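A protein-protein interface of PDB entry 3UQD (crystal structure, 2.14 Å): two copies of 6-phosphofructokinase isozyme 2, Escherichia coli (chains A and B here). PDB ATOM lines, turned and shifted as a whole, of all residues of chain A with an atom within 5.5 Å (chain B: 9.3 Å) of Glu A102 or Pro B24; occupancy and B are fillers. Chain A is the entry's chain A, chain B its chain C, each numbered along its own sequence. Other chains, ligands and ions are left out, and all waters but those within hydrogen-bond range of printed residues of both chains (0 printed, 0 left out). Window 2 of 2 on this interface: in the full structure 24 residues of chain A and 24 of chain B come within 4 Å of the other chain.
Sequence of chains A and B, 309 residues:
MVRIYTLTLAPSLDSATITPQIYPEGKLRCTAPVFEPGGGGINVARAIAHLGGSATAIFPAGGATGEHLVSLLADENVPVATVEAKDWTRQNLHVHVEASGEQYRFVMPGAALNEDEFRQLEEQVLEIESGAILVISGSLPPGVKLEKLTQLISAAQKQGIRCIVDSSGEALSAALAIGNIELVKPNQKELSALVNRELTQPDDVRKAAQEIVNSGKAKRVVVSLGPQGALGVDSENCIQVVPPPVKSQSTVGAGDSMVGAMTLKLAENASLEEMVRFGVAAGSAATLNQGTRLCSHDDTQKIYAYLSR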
ATOM      1  N   VAL A  95      -4.811 -24.709 -13.267  1.00  0.00           N
ATOM      2  CA  VAL A  95      -5.470 -25.806 -12.563  1.00  0.00           C
ATOM      3  C   VAL A  95      -5.524 -25.590 -11.048  1.00  0.00           C
ATOM      4  O   VAL A  95      -4.493 -25.458 -10.399  1.00  0.00           O
ATOM      5  CB  VAL A  95      -4.776 -27.154 -12.861  1.00  0.00           C
ATOM      6  CG1 VAL A  95      -5.473 -28.292 -12.129  1.00  0.00           C
ATOM      7  CG2 VAL A  95      -4.763 -27.418 -14.358  1.00  0.00           C
ATOM      8  N   HIS A  96      -6.733 -25.555 -10.494  1.00  0.00           N
ATOM      9  CA  HIS A  96      -6.924 -25.385  -9.056  1.00  0.00           C
ATOM     10  C   HIS A  96      -7.254 -26.725  -8.396  1.00  0.00           C
ATOM     11  O   HIS A  96      -8.272 -27.341  -8.710  1.00  0.00           O
ATOM     12  CB  HIS A  96      -8.046 -24.372  -8.787  1.00  0.00           C
ATOM     13  CG  HIS A  96      -8.353 -24.179  -7.331  1.00  0.00           C
ATOM     14  ND1 HIS A  96      -7.602 -23.361  -6.515  1.00  0.00           N
ATOM     15  CD2 HIS A  96      -9.325 -24.704  -6.548  1.00  0.00           C
ATOM     16  CE1 HIS A  96      -8.101 -23.387  -5.290  1.00  0.00           C
ATOM     17  NE2 HIS A  96      -9.145 -24.196  -5.282  1.00  0.00           N
ATOM     18  N   VAL A  97      -6.397 -27.178  -7.486  1.00  0.00           N
ATOM     19  CA  VAL A  97      -6.613 -28.453  -6.799  1.00  0.00           C
ATOM     20  C   VAL A  97      -7.361 -28.277  -5.476  1.00  0.00           C
ATOM     21  O   VAL A  97      -6.864 -27.635  -4.554  1.00  0.00           O
ATOM     22  CB  VAL A  97      -5.284 -29.195  -6.542  1.00  0.00           C
ATOM     23  CG1 VAL A  97      -5.542 -30.503  -5.808  1.00  0.00           C
ATOM     24  CG2 VAL A  97      -4.557 -29.450  -7.853  1.00  0.00           C
ATOM     25  N   SER A 100      -6.013 -29.458  -1.742  1.00  0.00           N
ATOM     26  CA  SER A 100      -4.947 -28.657  -1.148  1.00  0.00           C
ATOM     27  C   SER A 100      -5.177 -27.151  -1.266  1.00  0.00           C
ATOM     28  O   SER A 100      -4.683 -26.381  -0.444  1.00  0.00           O
ATOM     29  CB  SER A 100      -3.609 -29.020  -1.789  1.00  0.00           C
ATOM     30  OG  SER A 100      -3.663 -28.840  -3.193  1.00  0.00           O
ATOM     31  N   GLY A 101      -5.915 -26.730  -2.288  1.00  0.00           N
ATOM     32  CA  GLY A 101      -6.141 -25.312  -2.523  1.00  0.00           C
ATOM     33  C   GLY A 101      -5.026 -24.661  -3.325  1.00  0.00           C
ATOM     34  O   GLY A 101      -4.998 -23.446  -3.494  1.00  0.00           O
ATOM     35  N   GLU A 102      -4.100 -25.479  -3.816  1.00  0.00           N
ATOM     36  CA  GLU A 102      -2.971 -24.995  -4.600  1.00  0.00           C
ATOM     37  C   GLU A 102      -3.408 -24.767  -6.039  1.00  0.00           C
ATOM     38  O   GLU A 102      -4.434 -25.293  -6.465  1.00  0.00           O
ATOM     39  CB  GLU A 102      -1.831 -26.016  -4.568  1.00  0.00           C
ATOM     40  CG  GLU A 102      -1.419 -26.464  -3.174  1.00  0.00           C
ATOM     41  CD  GLU A 102      -0.637 -25.407  -2.415  1.00  0.00           C
ATOM     42  OE1 GLU A 102      -0.136 -24.454  -3.051  1.00  0.00           O
ATOM     43  OE2 GLU A 102      -0.520 -25.532  -1.177  1.00  0.00           O
ATOM     44  N   GLN A 103      -2.635 -23.984  -6.786  1.00  0.00           N
ATOM     45  CA  GLN A 103      -2.949 -23.733  -8.192  1.00  0.00           C
ATOM     46  C   GLN A 103      -1.723 -23.971  -9.062  1.00  0.00           C
ATOM     47  O   GLN A 103      -0.601 -23.723  -8.638  1.00  0.00           O
ATOM     48  CB  GLN A 103      -3.512 -22.316  -8.397  1.00  0.00           C
ATOM     49  CG  GLN A 103      -2.532 -21.199  -8.085  1.00  0.00           C
ATOM     50  CD  GLN A 103      -3.177 -19.823  -8.082  1.00  0.00           C
ATOM     51  OE1 GLN A 103      -4.074 -19.533  -8.875  1.00  0.00           O
ATOM     52  NE2 GLN A 103      -2.724 -18.968  -7.177  1.00  0.00           N
ATOM     53  N   TYR A 104      -1.945 -24.464 -10.274  1.00  0.00           N
ATOM     54  CA  TYR A 104      -0.854 -24.823 -11.178  1.00  0.00           C
ATOM     55  C   TYR A 104      -1.030 -24.145 -12.526  1.00  0.00           C
ATOM     56  O   TYR A 104      -2.112 -24.177 -13.109  1.00  0.00           O
ATOM     57  CB  TYR A 104      -0.768 -26.349 -11.346  1.00  0.00           C
ATOM     58  CG  TYR A 104      -0.342 -27.055 -10.077  1.00  0.00           C
ATOM     59  CD1 TYR A 104      -1.266 -27.367  -9.089  1.00  0.00           C
ATOM     60  CD2 TYR A 104       0.988 -27.383  -9.857  1.00  0.00           C
ATOM     61  CE1 TYR A 104      -0.881 -27.998  -7.921  1.00  0.00           C
ATOM     62  CE2 TYR A 104       1.389 -28.014  -8.685  1.00  0.00           C
ATOM     63  CZ  TYR A 104       0.449 -28.320  -7.722  1.00  0.00           C
ATOM     64  OH  TYR A 104       0.836 -28.945  -6.557  1.00  0.00           O
ATOM     65  N   GLN B  21      10.057 -29.069 -14.415  1.00  0.00           N
ATOM     66  CA  GLN B  21       9.539 -29.615 -13.166  1.00  0.00           C
ATOM     67  C   GLN B  21       8.135 -29.119 -12.839  1.00  0.00           C
ATOM     68  O   GLN B  21       7.580 -28.273 -13.547  1.00  0.00           O
ATOM     69  CB  GLN B  21      10.501 -29.340 -12.008  1.00  0.00           C
ATOM     70  CG  GLN B  21      10.964 -27.901 -11.898  1.00  0.00           C
ATOM     71  CD  GLN B  21      12.036 -27.720 -10.838  1.00  0.00           C
ATOM     72  OE1 GLN B  21      12.384 -28.662 -10.123  1.00  0.00           O
ATOM     73  NE2 GLN B  21      12.565 -26.506 -10.731  1.00  0.00           N
ATOM     74  N   ILE B  22       7.563 -29.661 -11.767  1.00  0.00           N
ATOM     75  CA  ILE B  22       6.199 -29.324 -11.383  1.00  0.00           C
ATOM     76  C   ILE B  22       6.101 -28.835  -9.936  1.00  0.00           C
ATOM     77  O   ILE B  22       6.627 -29.461  -9.008  1.00  0.00           O
ATOM     78  CB  ILE B  22       5.228 -30.501 -11.650  1.00  0.00           C
ATOM     79  CG1 ILE B  22       3.795 -30.117 -11.278  1.00  0.00           C
ATOM     80  CG2 ILE B  22       5.681 -31.757 -10.918  1.00  0.00           C
ATOM     81  CD1 ILE B  22       2.737 -30.976 -11.956  1.00  0.00           C
ATOM     82  N   TYR B  23       5.441 -27.695  -9.768  1.00  0.00           N
ATOM     83  CA  TYR B  23       5.257 -27.067  -8.465  1.00  0.00           C
ATOM     84  C   TYR B  23       4.162 -26.002  -8.565  1.00  0.00           C
ATOM     85  O   TYR B  23       3.841 -25.548  -9.662  1.00  0.00           O
ATOM     86  CB  TYR B  23       6.579 -26.473  -7.960  1.00  0.00           C
ATOM     87  CG  TYR B  23       7.256 -25.504  -8.906  1.00  0.00           C
ATOM     88  CD1 TYR B  23       6.890 -24.164  -8.941  1.00  0.00           C
ATOM     89  CD2 TYR B  23       8.278 -25.924  -9.748  1.00  0.00           C
ATOM     90  CE1 TYR B  23       7.513 -23.272  -9.794  1.00  0.00           C
ATOM     91  CE2 TYR B  23       8.908 -25.038 -10.603  1.00  0.00           C
ATOM     92  CZ  TYR B  23       8.521 -23.712 -10.622  1.00  0.00           C
ATOM     93  OH  TYR B  23       9.141 -22.824 -11.473  1.00  0.00           O
ATOM     94  N   PRO B  24       3.572 -25.607  -7.426  1.00  0.00           N
ATOM     95  CA  PRO B  24       2.424 -24.702  -7.505  1.00  0.00           C
ATOM     96  C   PRO B  24       2.807 -23.226  -7.600  1.00  0.00           C
ATOM     97  O   PRO B  24       3.983 -22.878  -7.465  1.00  0.00           O
ATOM     98  CB  PRO B  24       1.683 -24.953  -6.180  1.00  0.00           C
ATOM     99  CG  PRO B  24       2.424 -26.069  -5.482  1.00  0.00           C
ATOM    100  CD  PRO B  24       3.799 -26.071  -6.049  1.00  0.00           C
ATOM    101  N   GLU B  25       1.797 -22.393  -7.857  1.00  0.00           N
ATOM    102  CA  GLU B  25       1.920 -20.932  -7.858  1.00  0.00           C
ATOM    103  C   GLU B  25       2.761 -20.343  -9.000  1.00  0.00           C
ATOM    104  O   GLU B  25       2.329 -19.405  -9.667  1.00  0.00           O
ATOM    105  CB  GLU B  25       2.413 -20.420  -6.497  1.00  0.00           C
ATOM    106  CG  GLU B  25       2.161 -18.935  -6.257  1.00  0.00           C
ATOM    107  CD  GLU B  25       0.712 -18.623  -5.924  1.00  0.00           C
ATOM    108  OE1 GLU B  25       0.405 -17.442  -5.661  1.00  0.00           O
ATOM    109  OE2 GLU B  25      -0.119 -19.556  -5.915  1.00  0.00           O
ATOM    110  N   GLY B  26       3.955 -20.879  -9.224  1.00  0.00           N
ATOM    111  CA  GLY B  26       4.820 -20.358 -10.272  1.00  0.00           C
ATOM    112  C   GLY B  26       4.356 -20.696 -11.681  1.00  0.00           C
ATOM    113  O   GLY B  26       3.502 -21.558 -11.865  1.00  0.00           O
ATOM    114  N   LYS B  27       4.914 -20.011 -12.678  1.00  0.00           N
ATOM    115  CA  LYS B  27       4.665 -20.351 -14.076  1.00  0.00           C
ATOM    116  C   LYS B  27       5.499 -21.557 -14.484  1.00  0.00           C
ATOM    117  O   LYS B  27       6.724 -21.538 -14.376  1.00  0.00           O
ATOM    118  CB  LYS B  27       5.015 -19.183 -15.003  1.00  0.00           C
ATOM    119  CG  LYS B  27       4.125 -17.961 -14.882  1.00  0.00           C
ATOM    120  CD  LYS B  27       4.486 -16.929 -15.946  1.00  0.00           C
ATOM    121  CE  LYS B  27       3.648 -15.672 -15.805  1.00  0.00           C
ATOM    122  NZ  LYS B  27       3.971 -14.651 -16.842  1.00  0.00           N
ATOM    123  N   LEU B  28       4.840 -22.602 -14.965  1.00  0.00           N
ATOM    124  CA  LEU B  28       5.549 -23.771 -15.459  1.00  0.00           C
ATOM    125  C   LEU B  28       5.650 -23.713 -16.979  1.00  0.00           C
ATOM    126  O   LEU B  28       4.688 -24.019 -17.682  1.00  0.00           O
ATOM    127  CB  LEU B  28       4.840 -25.057 -15.032  1.00  0.00           C
ATOM    128  CG  LEU B  28       4.474 -25.173 -13.552  1.00  0.00           C
ATOM    129  CD1 LEU B  28       3.863 -26.532 -13.277  1.00  0.00           C
ATOM    130  CD2 LEU B  28       5.693 -24.942 -12.678  1.00  0.00           C
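O of Gln A103 sits at hydrogen-bond distance from N of Glu B25, 2.9 Å away.
N of Tyr A104 lies within hydrogen-bond range of O of Val A95 (2.7 Å).
The backbone carbonyl oxygen (O) of Glu A102 lies within hydrogen-bond range of the backbone NH (N) of Val A97 (2.9 Å).
OG of Ser A100 sits close to N of Glu A102.
Among the printed residues, pairs that only touch across the chains: Glu A102 with Pro B24 (3.7 Å), Gln A103 with Pro B24 (3.4 Å), Tyr A104 with Tyr B23 (3.4 Å) and Tyr A104 with Pro B24 (3.5 Å).
No residue of chain B comes within 4 Å of His A96.
Of the printed residues of chain B, Glu A102 touches Pro B24.
Of the printed residues of chain B, Tyr A104 touches Tyr B23 (3.4 Å) and Pro B24 (3.5 Å).
Printed residues of chain A within 4 Å of Tyr B23: Tyr A104 (3.4 Å).
The nearest printed residue of chain B that does not touch Glu A102 is Glu B25 (5.6 Å).
The nearest printed residue of chain A that does not touch Tyr B23 is Gln A103 (4.9 Å).
Of the 8 printed residues of chain B, 3 touch a printed residue of chain A.
Printed residues of chain B that touch a printed residue of chain A: Tyr B23, Pro B24 and Glu B25.
Among the printed residues, 5 pairs touch across the chains.
No position is printed for both chains.
Of the 5 pairs that touch across the chains among the printed residues, none has its exchanged pair printed and touching as well.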
